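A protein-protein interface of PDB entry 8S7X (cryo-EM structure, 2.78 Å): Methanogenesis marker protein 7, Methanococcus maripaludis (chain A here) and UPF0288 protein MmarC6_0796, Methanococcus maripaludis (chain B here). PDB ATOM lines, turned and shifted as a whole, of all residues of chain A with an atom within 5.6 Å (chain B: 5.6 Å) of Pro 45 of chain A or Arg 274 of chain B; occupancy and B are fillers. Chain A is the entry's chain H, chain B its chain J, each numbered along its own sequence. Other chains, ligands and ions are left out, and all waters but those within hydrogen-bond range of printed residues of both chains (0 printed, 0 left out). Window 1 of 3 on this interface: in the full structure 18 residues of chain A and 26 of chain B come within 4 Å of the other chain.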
ATOM      1  N   MET A   1       6.177 -30.308  21.561  1.00  0.00           N
ATOM      2  CA  MET A   1       6.358 -29.032  22.243  1.00  0.00           C
ATOM      3  C   MET A   1       7.090 -28.067  21.316  1.00  0.00           C
ATOM      4  O   MET A   1       6.600 -26.980  21.015  1.00  0.00           O
ATOM      5  CB  MET A   1       7.136 -29.221  23.547  1.00  0.00           C
ATOM      6  CG  MET A   1       7.456 -27.940  24.308  1.00  0.00           C
ATOM      7  SD  MET A   1       6.238 -26.620  24.104  1.00  0.00           S
ATOM      8  CE  MET A   1       6.509 -25.676  25.603  1.00  0.00           C
ATOM      9  N   TYR A   2       8.268 -28.484  20.863  1.00  0.00           N
ATOM     10  CA  TYR A   2       9.136 -27.668  20.022  1.00  0.00           C
ATOM     11  C   TYR A   2       8.893 -28.074  18.576  1.00  0.00           C
ATOM     12  O   TYR A   2       9.386 -29.111  18.128  1.00  0.00           O
ATOM     13  CB  TYR A   2      10.597 -27.883  20.403  1.00  0.00           C
ATOM     14  CG  TYR A   2      11.003 -27.277  21.722  1.00  0.00           C
ATOM     15  CD1 TYR A   2      11.035 -25.903  21.904  1.00  0.00           C
ATOM     16  CD2 TYR A   2      11.349 -28.086  22.791  1.00  0.00           C
ATOM     17  CE1 TYR A   2      11.407 -25.357  23.112  1.00  0.00           C
ATOM     18  CE2 TYR A   2      11.718 -27.549  24.001  1.00  0.00           C
ATOM     19  CZ  TYR A   2      11.745 -26.184  24.159  1.00  0.00           C
ATOM     20  OH  TYR A   2      12.114 -25.647  25.370  1.00  0.00           O
ATOM     21  N   GLN A   3       8.136 -27.271  17.834  1.00  0.00           N
ATOM     22  CA  GLN A   3       7.951 -27.569  16.422  1.00  0.00           C
ATOM     23  C   GLN A   3       9.008 -26.841  15.605  1.00  0.00           C
ATOM     24  O   GLN A   3       9.298 -25.664  15.838  1.00  0.00           O
ATOM     25  CB  GLN A   3       6.542 -27.219  15.945  1.00  0.00           C
ATOM     26  CG  GLN A   3       6.350 -25.829  15.388  1.00  0.00           C
ATOM     27  CD  GLN A   3       5.164 -25.757  14.450  1.00  0.00           C
ATOM     28  OE1 GLN A   3       4.518 -24.717  14.336  1.00  0.00           O
ATOM     29  NE2 GLN A   3       4.857 -26.861  13.789  1.00  0.00           N
ATOM     30  N   VAL A  24      12.698 -16.174  23.943  1.00  0.00           N
ATOM     31  CA  VAL A  24      11.514 -17.017  24.111  1.00  0.00           C
ATOM     32  C   VAL A  24      11.858 -18.484  24.295  1.00  0.00           C
ATOM     33  O   VAL A  24      10.948 -19.298  24.486  1.00  0.00           O
ATOM     34  CB  VAL A  24      10.536 -16.883  22.928  1.00  0.00           C
ATOM     35  CG1 VAL A  24      10.215 -15.427  22.677  1.00  0.00           C
ATOM     36  CG2 VAL A  24      11.113 -17.529  21.692  1.00  0.00           C
ATOM     37  N   GLY A  25      13.132 -18.848  24.245  1.00  0.00           N
ATOM     38  CA  GLY A  25      13.543 -20.204  24.534  1.00  0.00           C
ATOM     39  C   GLY A  25      13.714 -21.115  23.343  1.00  0.00           C
ATOM     40  O   GLY A  25      13.845 -22.329  23.533  1.00  0.00           O
ATOM     41  N   GLY A  26      13.718 -20.584  22.127  1.00  0.00           N
ATOM     42  CA  GLY A  26      13.939 -21.413  20.963  1.00  0.00           C
ATOM     43  C   GLY A  26      15.403 -21.750  20.754  1.00  0.00           C
ATOM     44  O   GLY A  26      16.296 -21.250  21.434  1.00  0.00           O
ATOM     45  N   ALA A  43      13.801 -24.329  16.171  1.00  0.00           N
ATOM     46  CA  ALA A  43      12.867 -25.111  16.971  1.00  0.00           C
ATOM     47  C   ALA A  43      12.405 -24.245  18.135  1.00  0.00           C
ATOM     48  O   ALA A  43      13.189 -23.950  19.040  1.00  0.00           O
ATOM     49  CB  ALA A  43      13.516 -26.396  17.470  1.00  0.00           C
ATOM     50  N   ILE A  44      11.139 -23.844  18.116  1.00  0.00           N
ATOM     51  CA  ILE A  44      10.594 -22.971  19.153  1.00  0.00           C
ATOM     52  C   ILE A  44       9.359 -23.633  19.749  1.00  0.00           C
ATOM     53  O   ILE A  44       8.717 -24.478  19.106  1.00  0.00           O
ATOM     54  CB  ILE A  44      10.266 -21.563  18.601  1.00  0.00           C
ATOM     55  CG1 ILE A  44       8.936 -21.564  17.867  1.00  0.00           C
ATOM     56  CG2 ILE A  44      11.359 -21.066  17.686  1.00  0.00           C
ATOM     57  CD1 ILE A  44       8.233 -20.242  17.941  1.00  0.00           C
ATOM     58  N   PRO A  45       9.005 -23.281  20.987  1.00  0.00           N
ATOM     59  CA  PRO A  45       7.818 -23.879  21.612  1.00  0.00           C
ATOM     60  C   PRO A  45       6.551 -23.544  20.840  1.00  0.00           C
ATOM     61  O   PRO A  45       6.446 -22.495  20.203  1.00  0.00           O
ATOM     62  CB  PRO A  45       7.797 -23.254  23.010  1.00  0.00           C
ATOM     63  CG  PRO A  45       9.179 -22.779  23.243  1.00  0.00           C
ATOM     64  CD  PRO A  45       9.719 -22.388  21.914  1.00  0.00           C
ATOM     65  N   GLN A  46       5.577 -24.457  20.909  1.00  0.00           N
ATOM     66  CA  GLN A  46       4.355 -24.288  20.129  1.00  0.00           C
ATOM     67  C   GLN A  46       3.555 -23.070  20.567  1.00  0.00           C
ATOM     68  O   GLN A  46       2.878 -22.447  19.743  1.00  0.00           O
ATOM     69  CB  GLN A  46       3.484 -25.540  20.214  1.00  0.00           C
ATOM     70  CG  GLN A  46       3.672 -26.497  19.052  1.00  0.00           C
ATOM     71  CD  GLN A  46       3.793 -27.938  19.490  1.00  0.00           C
ATOM     72  OE1 GLN A  46       3.740 -28.240  20.681  1.00  0.00           O
ATOM     73  NE2 GLN A  46       3.952 -28.838  18.528  1.00  0.00           N
ATOM     74  N   ASN A  47       3.615 -22.707  21.848  1.00  0.00           N
ATOM     75  CA  ASN A  47       2.840 -21.566  22.318  1.00  0.00           C
ATOM     76  C   ASN A  47       3.367 -20.238  21.793  1.00  0.00           C
ATOM     77  O   ASN A  47       2.697 -19.215  21.973  1.00  0.00           O
ATOM     78  CB  ASN A  47       2.804 -21.542  23.846  1.00  0.00           C
ATOM     79  CG  ASN A  47       4.136 -21.886  24.464  1.00  0.00           C
ATOM     80  OD1 ASN A  47       4.616 -23.012  24.344  1.00  0.00           O
ATOM     81  ND2 ASN A  47       4.742 -20.918  25.137  1.00  0.00           N
ATOM     82  N   GLU A  48       4.534 -20.226  21.153  1.00  0.00           N
ATOM     83  CA  GLU A  48       5.106 -19.008  20.594  1.00  0.00           C
ATOM     84  C   GLU A  48       5.122 -19.007  19.071  1.00  0.00           C
ATOM     85  O   GLU A  48       5.810 -18.176  18.473  1.00  0.00           O
ATOM     86  CB  GLU A  48       6.522 -18.803  21.128  1.00  0.00           C
ATOM     87  CG  GLU A  48       6.578 -18.536  22.616  1.00  0.00           C
ATOM     88  CD  GLU A  48       6.527 -17.063  22.949  1.00  0.00           C
ATOM     89  OE1 GLU A  48       5.797 -16.317  22.267  1.00  0.00           O
ATOM     90  OE2 GLU A  48       7.218 -16.644  23.898  1.00  0.00           O
ATOM     91  N   ILE A  49       4.374 -19.906  18.430  1.00  0.00           N
ATOM     92  CA  ILE A  49       4.411 -20.008  16.972  1.00  0.00           C
ATOM     93  C   ILE A  49       3.810 -18.764  16.325  1.00  0.00           C
ATOM     94  O   ILE A  49       4.388 -18.189  15.398  1.00  0.00           O
ATOM     95  CB  ILE A  49       3.698 -21.287  16.510  1.00  0.00           C
ATOM     96  CG1 ILE A  49       4.593 -22.492  16.758  1.00  0.00           C
ATOM     97  CG2 ILE A  49       3.344 -21.196  15.044  1.00  0.00           C
ATOM     98  CD1 ILE A  49       5.949 -22.356  16.120  1.00  0.00           C
ATOM     99  N   THR B 230       5.801 -16.738  27.046  1.00  0.00           N
ATOM    100  CA  THR B 230       6.793 -17.300  27.949  1.00  0.00           C
ATOM    101  C   THR B 230       7.386 -16.312  28.937  1.00  0.00           C
ATOM    102  O   THR B 230       7.929 -16.752  29.955  1.00  0.00           O
ATOM    103  CB  THR B 230       7.946 -17.933  27.156  1.00  0.00           C
ATOM    104  OG1 THR B 230       8.630 -16.920  26.415  1.00  0.00           O
ATOM    105  CG2 THR B 230       7.427 -18.989  26.203  1.00  0.00           C
ATOM    106  N   ASP B 249      18.859 -22.544  34.775  1.00  0.00           N
ATOM    107  CA  ASP B 249      17.557 -22.760  34.161  1.00  0.00           C
ATOM    108  C   ASP B 249      16.633 -21.576  34.401  1.00  0.00           C
ATOM    109  O   ASP B 249      16.543 -21.054  35.515  1.00  0.00           O
ATOM    110  CB  ASP B 249      16.929 -24.036  34.714  1.00  0.00           C
ATOM    111  CG  ASP B 249      17.354 -25.271  33.952  1.00  0.00           C
ATOM    112  OD1 ASP B 249      18.520 -25.322  33.512  1.00  0.00           O
ATOM    113  OD2 ASP B 249      16.525 -26.189  33.797  1.00  0.00           O
ATOM    114  N   ARG B 250      15.948 -21.152  33.340  1.00  0.00           N
ATOM    115  CA  ARG B 250      14.945 -20.094  33.430  1.00  0.00           C
ATOM    116  C   ARG B 250      13.604 -20.752  33.733  1.00  0.00           C
ATOM    117  O   ARG B 250      12.749 -20.940  32.867  1.00  0.00           O
ATOM    118  CB  ARG B 250      14.906 -19.281  32.145  1.00  0.00           C
ATOM    119  CG  ARG B 250      16.219 -18.605  31.813  1.00  0.00           C
ATOM    120  CD  ARG B 250      16.162 -17.922  30.464  1.00  0.00           C
ATOM    121  NE  ARG B 250      16.301 -18.870  29.366  1.00  0.00           N
ATOM    122  CZ  ARG B 250      16.143 -18.558  28.086  1.00  0.00           C
ATOM    123  NH1 ARG B 250      15.829 -17.332  27.711  1.00  0.00           N
ATOM    124  NH2 ARG B 250      16.304 -19.501  27.166  1.00  0.00           N
ATOM    125  N   ASP B 251      13.423 -21.108  35.001  1.00  0.00           N
ATOM    126  CA  ASP B 251      12.259 -21.867  35.428  1.00  0.00           C
ATOM    127  C   ASP B 251      11.040 -20.955  35.516  1.00  0.00           C
ATOM    128  O   ASP B 251      11.070 -19.786  35.124  1.00  0.00           O
ATOM    129  CB  ASP B 251      12.533 -22.555  36.762  1.00  0.00           C
ATOM    130  CG  ASP B 251      13.755 -23.439  36.719  1.00  0.00           C
ATOM    131  OD1 ASP B 251      13.807 -24.339  35.856  1.00  0.00           O
ATOM    132  OD2 ASP B 251      14.665 -23.237  37.551  1.00  0.00           O
ATOM    133  N   TYR B 270       9.924 -14.997  33.729  1.00  0.00           N
ATOM    134  CA  TYR B 270       9.531 -16.102  32.868  1.00  0.00           C
ATOM    135  C   TYR B 270       8.299 -16.806  33.418  1.00  0.00           C
ATOM    136  O   TYR B 270       8.265 -17.195  34.587  1.00  0.00           O
ATOM    137  CB  TYR B 270      10.684 -17.096  32.720  1.00  0.00           C
ATOM    138  CG  TYR B 270      11.626 -16.748  31.594  1.00  0.00           C
ATOM    139  CD1 TYR B 270      12.654 -15.843  31.782  1.00  0.00           C
ATOM    140  CD2 TYR B 270      11.474 -17.314  30.340  1.00  0.00           C
ATOM    141  CE1 TYR B 270      13.511 -15.520  30.756  1.00  0.00           C
ATOM    142  CE2 TYR B 270      12.326 -16.997  29.311  1.00  0.00           C
ATOM    143  CZ  TYR B 270      13.342 -16.099  29.523  1.00  0.00           C
ATOM    144  OH  TYR B 270      14.191 -15.783  28.493  1.00  0.00           O
ATOM    145  N   GLU B 272       7.189 -19.614  31.891  1.00  0.00           N
ATOM    146  CA  GLU B 272       7.294 -20.995  31.455  1.00  0.00           C
ATOM    147  C   GLU B 272       8.685 -21.518  31.777  1.00  0.00           C
ATOM    148  O   GLU B 272       9.655 -20.761  31.813  1.00  0.00           O
ATOM    149  CB  GLU B 272       7.024 -21.135  29.956  1.00  0.00           C
ATOM    150  CG  GLU B 272       5.648 -20.669  29.535  1.00  0.00           C
ATOM    151  CD  GLU B 272       4.664 -21.807  29.398  1.00  0.00           C
ATOM    152  OE1 GLU B 272       5.107 -22.949  29.157  1.00  0.00           O
ATOM    153  OE2 GLU B 272       3.448 -21.559  29.539  1.00  0.00           O
ATOM    154  N   SER B 273       8.773 -22.827  31.999  1.00  0.00           N
ATOM    155  CA  SER B 273      10.047 -23.467  32.302  1.00  0.00           C
ATOM    156  C   SER B 273      10.826 -23.634  31.005  1.00  0.00           C
ATOM    157  O   SER B 273      10.435 -24.413  30.132  1.00  0.00           O
ATOM    158  CB  SER B 273       9.824 -24.812  32.986  1.00  0.00           C
ATOM    159  OG  SER B 273       9.231 -24.647  34.261  1.00  0.00           O
ATOM    160  N   ARG B 274      11.927 -22.902  30.874  1.00  0.00           N
ATOM    161  CA  ARG B 274      12.754 -22.924  29.680  1.00  0.00           C
ATOM    162  C   ARG B 274      14.183 -23.309  30.042  1.00  0.00           C
ATOM    163  O   ARG B 274      14.540 -23.449  31.213  1.00  0.00           O
ATOM    164  CB  ARG B 274      12.732 -21.568  28.968  1.00  0.00           C
ATOM    165  CG  ARG B 274      11.352 -21.142  28.520  1.00  0.00           C
ATOM    166  CD  ARG B 274      11.152 -21.429  27.049  1.00  0.00           C
ATOM    167  NE  ARG B 274       9.748 -21.379  26.656  1.00  0.00           N
ATOM    168  CZ  ARG B 274       8.909 -22.402  26.747  1.00  0.00           C
ATOM    169  NH1 ARG B 274       9.297 -23.571  27.227  1.00  0.00           N
ATOM    170  NH2 ARG B 274       7.653 -22.247  26.347  1.00  0.00           N
ATOM    171  N   ALA B 275      15.001 -23.483  29.012  1.00  0.00           N
ATOM    172  CA  ALA B 275      16.378 -23.900  29.200  1.00  0.00           C
ATOM    173  C   ALA B 275      17.255 -22.717  29.593  1.00  0.00           C
ATOM    174  O   ALA B 275      16.876 -21.549  29.471  1.00  0.00           O
ATOM    175  CB  ALA B 275      16.913 -24.555  27.930  1.00  0.00           C
ATOM    176  N   SER B 276      18.453 -23.034  30.075  1.00  0.00           N
ATOM    177  CA  SER B 276      19.421 -22.008  30.429  1.00  0.00           C
ATOM    178  C   SER B 276      19.886 -21.260  29.185  1.00  0.00           C
ATOM    179  O   SER B 276      19.872 -21.789  28.072  1.00  0.00           O
ATOM    180  CB  SER B 276      20.618 -22.637  31.141  1.00  0.00           C
ATOM    181  OG  SER B 276      21.738 -21.776  31.108  1.00  0.00           O
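The backbone carbonyl oxygen of Val 24 of chain A sits at hydrogen-bond distance from the guanidinium group of Arg 274 of chain B, 3.2 Å away.
The side-chain amide nitrogen of Asn 47 of chain A sits close to the guanidinium group of Arg 274 of chain B (3.4 Å).
The side-chain hydroxyl (OG1) of Thr 230 of chain B is in hydrogen-bond range of the side-chain carboxylate (OE2) of Glu 48 of chain A.
Among the printed residues, pairs that only touch across the chains: Asn 47 of chain A with Thr 230 of chain B, Pro 45 of chain A with Arg 274 of chain B, Gly 25 of chain A with Arg 274 of chain B, Met 1 of chain A with Arg 274 of chain B, Val 24 of chain A with Thr 230 of chain B, Gly 25 of chain A with Arg 250 of chain B and Tyr 2 of chain A with Arg 274 of chain B.
Of the printed residues of chain B, Tyr 2 of chain A touches Arg 274 (3.96 Å).
Pro 45 of chain A touches just one residue of chain B: Arg 274.
Asp 249 of chain B touches none of the printed residues of chain A.
Of the printed residues of chain A, Arg 250 of chain B touches Gly 25 (3.9 Å).
Arg 274 of chain B touches six residues of chain A.
The nearest residue of chain A that does not touch Arg 274 of chain B is Glu 48 of chain A (5.4 Å).
The nearest printed residue of chain A that does not touch Arg 250 of chain B is Val 24 of chain A (5.0 Å).
Of the 13 printed residues of chain A, 7 touch a printed residue of chain B.
Printed residues of chain A that touch a printed residue of chain B: Met 1, Tyr 2, Val 24, Gly 25, Pro 45, Asn 47 and Glu 48.
Of the 10 printed residues of chain B, 3 touch a printed residue of chain A.
Among the printed residues, 10 pairs touch across the chains.
Among the printed residues, no Asp or Glu carboxylate lies within 4 Å of a Lys or Arg side-chain nitrogen of the other chain.
O of Met 1 of chain A lies within hydrogen-bond range of N of Gln 46 of chain A.
The backbone NH (N) of Arg 274 of chain B is in hydrogen-bond range of the backbone carbonyl oxygen (O) of Arg 250 of chain B (2.9 Å).
NE of Arg 250 of chain B is in hydrogen-bond range of O of Ala 275 of chain B, 2.7 Å away.
The guanidinium group of Arg 274 of chain B is in salt-bridge range of the side-chain carboxylate of Glu 272 of chain B.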
